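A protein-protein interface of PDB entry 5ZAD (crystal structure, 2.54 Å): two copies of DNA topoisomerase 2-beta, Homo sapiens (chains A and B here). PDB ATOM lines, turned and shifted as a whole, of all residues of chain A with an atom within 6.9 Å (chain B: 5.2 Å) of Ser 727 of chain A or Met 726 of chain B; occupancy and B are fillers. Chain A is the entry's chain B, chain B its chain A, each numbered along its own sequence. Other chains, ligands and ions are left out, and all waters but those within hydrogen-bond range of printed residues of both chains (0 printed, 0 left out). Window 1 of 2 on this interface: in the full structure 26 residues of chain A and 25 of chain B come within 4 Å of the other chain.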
ATOM      1  N   ILE A 653      -2.329  10.340  -3.851  1.00  0.00           N
ATOM      2  CA  ILE A 653      -2.784  11.180  -2.751  1.00  0.00           C
ATOM      3  C   ILE A 653      -4.284  11.442  -2.836  1.00  0.00           C
ATOM      4  O   ILE A 653      -5.004  11.325  -1.835  1.00  0.00           O
ATOM      5  CB  ILE A 653      -1.943  12.464  -2.723  1.00  0.00           C
ATOM      6  CG1 ILE A 653      -2.255  13.326  -1.536  1.00  0.00           C
ATOM      7  CG2 ILE A 653      -2.129  13.279  -3.967  1.00  0.00           C
ATOM      8  CD1 ILE A 653      -0.992  13.896  -1.059  1.00  0.00           C
ATOM      9  N   ILE A 723       6.483   8.438  -3.574  1.00  0.00           N
ATOM     10  CA  ILE A 723       5.168   8.680  -2.979  1.00  0.00           C
ATOM     11  C   ILE A 723       5.251   8.613  -1.463  1.00  0.00           C
ATOM     12  O   ILE A 723       4.646   9.425  -0.759  1.00  0.00           O
ATOM     13  CB  ILE A 723       4.087   7.701  -3.488  1.00  0.00           C
ATOM     14  CG1 ILE A 723       4.016   7.597  -5.009  1.00  0.00           C
ATOM     15  CG2 ILE A 723       2.746   8.066  -2.914  1.00  0.00           C
ATOM     16  CD1 ILE A 723       4.976   6.614  -5.572  1.00  0.00           C
ATOM     17  N   LEU A 724       5.968   7.627  -0.947  1.00  0.00           N
ATOM     18  CA  LEU A 724       5.856   7.245   0.447  1.00  0.00           C
ATOM     19  C   LEU A 724       6.778   8.041   1.352  1.00  0.00           C
ATOM     20  O   LEU A 724       6.428   8.290   2.510  1.00  0.00           O
ATOM     21  CB  LEU A 724       6.115   5.743   0.554  1.00  0.00           C
ATOM     22  CG  LEU A 724       4.897   4.826   0.577  1.00  0.00           C
ATOM     23  CD1 LEU A 724       4.216   5.033   1.895  1.00  0.00           C
ATOM     24  CD2 LEU A 724       3.933   5.096  -0.575  1.00  0.00           C
ATOM     25  N   ASN A 725       7.934   8.476   0.852  1.00  0.00           N
ATOM     26  CA  ASN A 725       8.717   9.437   1.610  1.00  0.00           C
ATOM     27  C   ASN A 725       8.056  10.809   1.661  1.00  0.00           C
ATOM     28  O   ASN A 725       8.535  11.680   2.400  1.00  0.00           O
ATOM     29  CB  ASN A 725      10.131   9.535   1.038  1.00  0.00           C
ATOM     30  CG  ASN A 725      11.031   8.413   1.531  1.00  0.00           C
ATOM     31  OD1 ASN A 725      10.766   7.794   2.562  1.00  0.00           O
ATOM     32  ND2 ASN A 725      12.102   8.147   0.796  1.00  0.00           N
ATOM     33  N   MET A 726       6.969  11.011   0.915  1.00  0.00           N
ATOM     34  CA  MET A 726       6.253  12.276   0.957  1.00  0.00           C
ATOM     35  C   MET A 726       5.866  12.618   2.384  1.00  0.00           C
ATOM     36  O   MET A 726       5.581  11.741   3.209  1.00  0.00           O
ATOM     37  CB  MET A 726       4.987  12.221   0.106  1.00  0.00           C
ATOM     38  CG  MET A 726       4.947  13.182  -1.065  1.00  0.00           C
ATOM     39  SD  MET A 726       3.351  13.106  -1.913  1.00  0.00           S
ATOM     40  CE  MET A 726       3.630  11.821  -3.125  1.00  0.00           C
ATOM     41  N   SER A 727       5.860  13.914   2.660  1.00  0.00           N
ATOM     42  CA  SER A 727       5.389  14.405   3.939  1.00  0.00           C
ATOM     43  C   SER A 727       3.997  13.863   4.233  1.00  0.00           C
ATOM     44  O   SER A 727       3.164  13.697   3.337  1.00  0.00           O
ATOM     45  CB  SER A 727       5.373  15.929   3.942  1.00  0.00           C
ATOM     46  OG  SER A 727       4.580  16.418   5.001  1.00  0.00           O
ATOM     47  N   LEU A 728       3.748  13.592   5.513  1.00  0.00           N
ATOM     48  CA  LEU A 728       2.388  13.305   5.950  1.00  0.00           C
ATOM     49  C   LEU A 728       1.466  14.485   5.679  1.00  0.00           C
ATOM     50  O   LEU A 728       0.252  14.298   5.539  1.00  0.00           O
ATOM     51  CB  LEU A 728       2.391  12.984   7.446  1.00  0.00           C
ATOM     52  CG  LEU A 728       1.219  12.250   8.080  1.00  0.00           C
ATOM     53  CD1 LEU A 728       1.017  10.959   7.345  1.00  0.00           C
ATOM     54  CD2 LEU A 728       1.487  11.987   9.563  1.00  0.00           C
ATOM     55  N   TRP A 729       2.031  15.693   5.601  1.00  0.00           N
ATOM     56  CA  TRP A 729       1.257  16.871   5.259  1.00  0.00           C
ATOM     57  C   TRP A 729       0.651  16.798   3.871  1.00  0.00           C
ATOM     58  O   TRP A 729      -0.288  17.531   3.585  1.00  0.00           O
ATOM     59  CB  TRP A 729       2.127  18.131   5.358  1.00  0.00           C
ATOM     60  CG  TRP A 729       1.396  19.287   5.904  1.00  0.00           C
ATOM     61  CD1 TRP A 729       0.279  19.848   5.393  1.00  0.00           C
ATOM     62  CD2 TRP A 729       1.710  20.021   7.083  1.00  0.00           C
ATOM     63  NE1 TRP A 729      -0.137  20.894   6.174  1.00  0.00           N
ATOM     64  CE2 TRP A 729       0.729  21.023   7.224  1.00  0.00           C
ATOM     65  CE3 TRP A 729       2.729  19.939   8.027  1.00  0.00           C
ATOM     66  CZ2 TRP A 729       0.733  21.927   8.277  1.00  0.00           C
ATOM     67  CZ3 TRP A 729       2.724  20.821   9.073  1.00  0.00           C
ATOM     68  CH2 TRP A 729       1.739  21.812   9.189  1.00  0.00           C
ATOM     69  N   SER A 730       1.144  15.937   2.995  1.00  0.00           N
ATOM     70  CA  SER A 730       0.773  16.097   1.596  1.00  0.00           C
ATOM     71  C   SER A 730      -0.726  15.923   1.345  1.00  0.00           C
ATOM     72  O   SER A 730      -1.248  16.430   0.335  1.00  0.00           O
ATOM     73  CB  SER A 730       1.593  15.145   0.747  1.00  0.00           C
ATOM     74  OG  SER A 730       2.785  15.748   0.258  1.00  0.00           O
ATOM     75  N   LEU A 731      -1.444  15.240   2.238  1.00  0.00           N
ATOM     76  CA  LEU A 731      -2.911  15.125   2.167  1.00  0.00           C
ATOM     77  C   LEU A 731      -3.631  16.053   3.144  1.00  0.00           C
ATOM     78  O   LEU A 731      -3.869  15.690   4.299  1.00  0.00           O
ATOM     79  CB  LEU A 731      -3.387  13.653   2.337  1.00  0.00           C
ATOM     80  CG  LEU A 731      -2.917  12.793   3.511  1.00  0.00           C
ATOM     81  CD1 LEU A 731      -3.517  11.597   4.264  1.00  0.00           C
ATOM     82  CD2 LEU A 731      -2.525  11.960   2.245  1.00  0.00           C
ATOM     83  N   LYS A 735      -2.408  21.431   0.626  1.00  0.00           N
ATOM     84  CA  LYS A 735      -1.273  20.828  -0.102  1.00  0.00           C
ATOM     85  C   LYS A 735      -1.688  19.942  -1.275  1.00  0.00           C
ATOM     86  O   LYS A 735      -0.842  19.656  -2.122  1.00  0.00           O
ATOM     87  CB  LYS A 735      -0.355  19.987   0.837  1.00  0.00           C
ATOM     88  CG  LYS A 735       0.238  20.649   2.111  1.00  0.00           C
ATOM     89  CD  LYS A 735       0.667  22.125   2.099  1.00  0.00           C
ATOM     90  CE  LYS A 735       2.145  22.303   1.753  1.00  0.00           C
ATOM     91  NZ  LYS A 735       2.727  23.298   2.691  1.00  0.00           N
ATOM     92  N   GLN B 649       3.977  12.390  18.895  1.00  0.00           N
ATOM     93  CA  GLN B 649       4.238  11.652  17.660  1.00  0.00           C
ATOM     94  C   GLN B 649       3.717  10.224  17.721  1.00  0.00           C
ATOM     95  O   GLN B 649       3.376   9.641  16.684  1.00  0.00           O
ATOM     96  CB  GLN B 649       5.738  11.650  17.351  1.00  0.00           C
ATOM     97  CG  GLN B 649       6.378  13.012  17.490  1.00  0.00           C
ATOM     98  CD  GLN B 649       7.629  13.169  16.676  1.00  0.00           C
ATOM     99  OE1 GLN B 649       7.900  14.242  16.141  1.00  0.00           O
ATOM    100  NE2 GLN B 649       8.410  12.098  16.577  1.00  0.00           N
ATOM    101  N   ILE B 653      -0.038   8.641  15.577  1.00  0.00           N
ATOM    102  CA  ILE B 653       0.014   7.598  14.558  1.00  0.00           C
ATOM    103  C   ILE B 653      -0.973   6.490  14.891  1.00  0.00           C
ATOM    104  O   ILE B 653      -1.698   6.000  14.015  1.00  0.00           O
ATOM    105  CB  ILE B 653       1.450   7.061  14.399  1.00  0.00           C
ATOM    106  CG1 ILE B 653       2.214   7.847  13.333  1.00  0.00           C
ATOM    107  CG2 ILE B 653       1.429   5.595  14.030  1.00  0.00           C
ATOM    108  CD1 ILE B 653       2.209   9.345  13.528  1.00  0.00           C
ATOM    109  N   ASN B 721       4.222  20.816  13.451  1.00  0.00           N
ATOM    110  CA  ASN B 721       4.876  20.301  12.254  1.00  0.00           C
ATOM    111  C   ASN B 721       5.604  18.998  12.527  1.00  0.00           C
ATOM    112  O   ASN B 721       5.772  18.181  11.613  1.00  0.00           O
ATOM    113  CB  ASN B 721       5.868  21.319  11.712  1.00  0.00           C
ATOM    114  CG  ASN B 721       5.192  22.488  11.075  1.00  0.00           C
ATOM    115  OD1 ASN B 721       4.925  22.487   9.877  1.00  0.00           O
ATOM    116  ND2 ASN B 721       4.904  23.504  11.873  1.00  0.00           N
ATOM    117  N   TYR B 722       6.050  18.793  13.766  1.00  0.00           N
ATOM    118  CA  TYR B 722       6.830  17.604  14.064  1.00  0.00           C
ATOM    119  C   TYR B 722       6.020  16.327  13.873  1.00  0.00           C
ATOM    120  O   TYR B 722       6.599  15.277  13.565  1.00  0.00           O
ATOM    121  CB  TYR B 722       7.405  17.695  15.477  1.00  0.00           C
ATOM    122  CG  TYR B 722       6.397  17.693  16.596  1.00  0.00           C
ATOM    123  CD1 TYR B 722       5.576  18.791  16.826  1.00  0.00           C
ATOM    124  CD2 TYR B 722       6.288  16.603  17.446  1.00  0.00           C
ATOM    125  CE1 TYR B 722       4.661  18.787  17.863  1.00  0.00           C
ATOM    126  CE2 TYR B 722       5.384  16.594  18.489  1.00  0.00           C
ATOM    127  CZ  TYR B 722       4.578  17.689  18.698  1.00  0.00           C
ATOM    128  OH  TYR B 722       3.667  17.669  19.729  1.00  0.00           O
ATOM    129  N   ILE B 723       4.689  16.385  14.025  1.00  0.00           N
ATOM    130  CA  ILE B 723       3.866  15.238  13.638  1.00  0.00           C
ATOM    131  C   ILE B 723       3.693  15.188  12.130  1.00  0.00           C
ATOM    132  O   ILE B 723       3.759  14.119  11.518  1.00  0.00           O
ATOM    133  CB  ILE B 723       2.476  15.226  14.316  1.00  0.00           C
ATOM    134  CG1 ILE B 723       2.514  15.351  15.839  1.00  0.00           C
ATOM    135  CG2 ILE B 723       1.706  13.988  13.899  1.00  0.00           C
ATOM    136  CD1 ILE B 723       2.568  16.750  16.312  1.00  0.00           C
ATOM    137  N   LEU B 724       3.414  16.330  11.520  1.00  0.00           N
ATOM    138  CA  LEU B 724       2.915  16.334  10.154  1.00  0.00           C
ATOM    139  C   LEU B 724       4.007  16.358   9.101  1.00  0.00           C
ATOM    140  O   LEU B 724       3.801  15.837   7.998  1.00  0.00           O
ATOM    141  CB  LEU B 724       1.965  17.504   9.959  1.00  0.00           C
ATOM    142  CG  LEU B 724       0.527  17.029   9.913  1.00  0.00           C
ATOM    143  CD1 LEU B 724      -0.343  18.183   9.486  1.00  0.00           C
ATOM    144  CD2 LEU B 724       0.420  15.844   8.956  1.00  0.00           C
ATOM    145  N   ASN B 725       5.163  16.944   9.400  1.00  0.00           N
ATOM    146  CA  ASN B 725       6.289  16.761   8.496  1.00  0.00           C
ATOM    147  C   ASN B 725       6.773  15.319   8.483  1.00  0.00           C
ATOM    148  O   ASN B 725       7.622  14.976   7.654  1.00  0.00           O
ATOM    149  CB  ASN B 725       7.431  17.705   8.880  1.00  0.00           C
ATOM    150  CG  ASN B 725       7.166  19.140   8.452  1.00  0.00           C
ATOM    151  OD1 ASN B 725       6.354  19.398   7.564  1.00  0.00           O
ATOM    152  ND2 ASN B 725       7.848  20.083   9.092  1.00  0.00           N
ATOM    153  N   MET B 726       6.228  14.473   9.362  1.00  0.00           N
ATOM    154  CA  MET B 726       6.589  13.065   9.409  1.00  0.00           C
ATOM    155  C   MET B 726       6.420  12.402   8.053  1.00  0.00           C
ATOM    156  O   MET B 726       5.572  12.786   7.241  1.00  0.00           O
ATOM    157  CB  MET B 726       5.728  12.318  10.424  1.00  0.00           C
ATOM    158  CG  MET B 726       6.477  11.713  11.585  1.00  0.00           C
ATOM    159  SD  MET B 726       5.382  10.700  12.596  1.00  0.00           S
ATOM    160  CE  MET B 726       4.828  11.869  13.827  1.00  0.00           C
ATOM    161  N   SER B 727       7.267  11.404   7.823  1.00  0.00           N
ATOM    162  CA  SER B 727       7.165  10.552   6.651  1.00  0.00           C
ATOM    163  C   SER B 727       5.751  10.007   6.498  1.00  0.00           C
ATOM    164  O   SER B 727       5.052   9.743   7.482  1.00  0.00           O
ATOM    165  CB  SER B 727       8.162   9.405   6.784  1.00  0.00           C
ATOM    166  OG  SER B 727       7.739   8.276   6.050  1.00  0.00           O
ATOM    167  N   LEU B 728       5.315   9.859   5.244  1.00  0.00           N
ATOM    168  CA  LEU B 728       4.073   9.131   4.991  1.00  0.00           C
ATOM    169  C   LEU B 728       4.172   7.677   5.424  1.00  0.00           C
ATOM    170  O   LEU B 728       3.144   7.063   5.728  1.00  0.00           O
ATOM    171  CB  LEU B 728       3.703   9.214   3.512  1.00  0.00           C
ATOM    172  CG  LEU B 728       2.210   9.166   3.214  1.00  0.00           C
ATOM    173  CD1 LEU B 728       1.525  10.311   3.925  1.00  0.00           C
ATOM    174  CD2 LEU B 728       1.957   9.233   1.716  1.00  0.00           C
ATOM    175  N   SER B 730       4.971   6.749   8.154  1.00  0.00           N
ATOM    176  CA  SER B 730       4.774   6.668   9.601  1.00  0.00           C
ATOM    177  C   SER B 730       3.612   5.755   9.982  1.00  0.00           C
ATOM    178  O   SER B 730       3.463   5.416  11.162  1.00  0.00           O
ATOM    179  CB  SER B 730       4.469   8.062  10.152  1.00  0.00           C
ATOM    180  OG  SER B 730       5.338   9.045   9.627  1.00  0.00           O
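Leu 724 of chain A touches Leu 728 of chain B, and with the chains exchanged Leu 728 of chain A touches Leu 724 of chain B. Met 726 of chain A touches Leu 728 of chain B, and with the chains exchanged Leu 728 of chain A touches Met 726 of chain B. Ser 727 of chain A touches Leu 728 of chain B, but with the chains exchanged Leu 728 of chain A does not touch Ser 727 of chain B (4.2 Å). Leu 728 of chain B touches its own counterpart, Leu 728 of chain A. 8 positions are printed for both chains. Of the 16 pairs that touch across the chains among the printed residues, 11 have their exchanged pair printed and touching as well.
OG of Ser 730 of chain B lies close to SD of Met 726 of chain B (3.4 Å). The side-chain hydroxyl (OG) of Ser 730 of chain A is in hydrogen-bond range of the side-chain sulfur (SD) of Met 726 of chain A. N of Trp 729 of chain A sits at hydrogen-bond distance from OG of Ser 727 of chain A (2.7 Å).
The backbone carbonyl oxygen (O) of Leu 724 of chain B is in hydrogen-bond range of the side-chain hydroxyl (OG) of Ser 727 of chain A (3.2 Å). N of Leu 728 of chain A lies close to O of Leu 724 of chain B (3.3 Å). The backbone carbonyl oxygen of Leu 724 of chain B sits at hydrogen-bond distance from the backbone NH of Trp 729 of chain A (3.0 Å). The backbone carbonyl oxygen of Met 726 of chain B sits at hydrogen-bond distance from the backbone NH of Leu 728 of chain A (2.6 Å). The backbone NH (N) of Leu 728 of chain B sits close to the backbone carbonyl oxygen (O) of Leu 724 of chain A (3.3 Å). O of Met 726 of chain A lies within hydrogen-bond range of N of Leu 728 of chain B, at 2.8 Å.
Of the printed residues of chain A, Met 726 of chain B touches Ser 727 (3.6 Å) and Leu 728 (2.6 Å). Printed residues of chain B within 4 Å of Met 726 of chain A: Ser 727 (3.7 Å) and Leu 728 (2.8 Å). Printed residues of chain B within 4 Å of Leu 724 of chain A: Ser 727 and Leu 728. Printed residues of chain A within 4 Å of Ile 723 of chain B: Leu 728. Printed residues of chain B within 4 Å of Leu 728 of chain A: Ile 723 (3.7 Å), Leu 724 (3.2 Å), Met 726 (2.6 Å) and Leu 728 (3.5 Å). Of the printed residues of chain B, Ile 723 of chain A touches Leu 728 (3.7 Å). Ile 653 of chain B touches none of the printed residues of chain A. The nearest residue of chain B that does not touch Ser 727 of chain A is Ser 727 of chain B (4.8 Å). The nearest residue of chain A that does not touch Met 726 of chain B is Met 726 of chain A (4.2 Å). The nearest printed residue of chain A that does not touch Ile 723 of chain B is Trp 729 of chain A (6.4 Å).
O of Ile 723 of chain A touches CD2 of Leu 728 of chain B, 3.7 Å away. O of Leu 724 of chain A touches OG of Ser 727 of chain B, at 3.8 Å. Ser 727 of chain B touches Met 726 of chain A. CA of Asn 725 of chain B touches OG of Ser 727 of chain A, 3.9 Å away. C of Ser 727 of chain A touches O of Met 726 of chain B, at 3.6 Å. Leu 728 of chain B touches Ser 727 of chain A (CD1 to O, 3.8 Å). Ile 723 of chain B touches Leu 728 of chain A. Leu 728 of chain B touches Leu 728 of chain A (CD1 to CD1, 3.5 Å). Trp 729 of chain A touches Asn 721 of chain B. Trp 729 of chain A touches Asn 725 of chain B.
Of the 11 printed residues of chain A, 6 touch a printed residue of chain B. Printed residues of chain A that touch a printed residue of chain B: Ile 723, Leu 724, Met 726, Ser 727, Leu 728 and Trp 729. Hydrophobic or aromatic side chains of chain A within 4 Å of the printed part of chain B: Leu 728 and Trp 729. Among the printed residues, no Asp or Glu carboxylate lies within 4 Å of a Lys or Arg side-chain nitrogen of the other chain.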
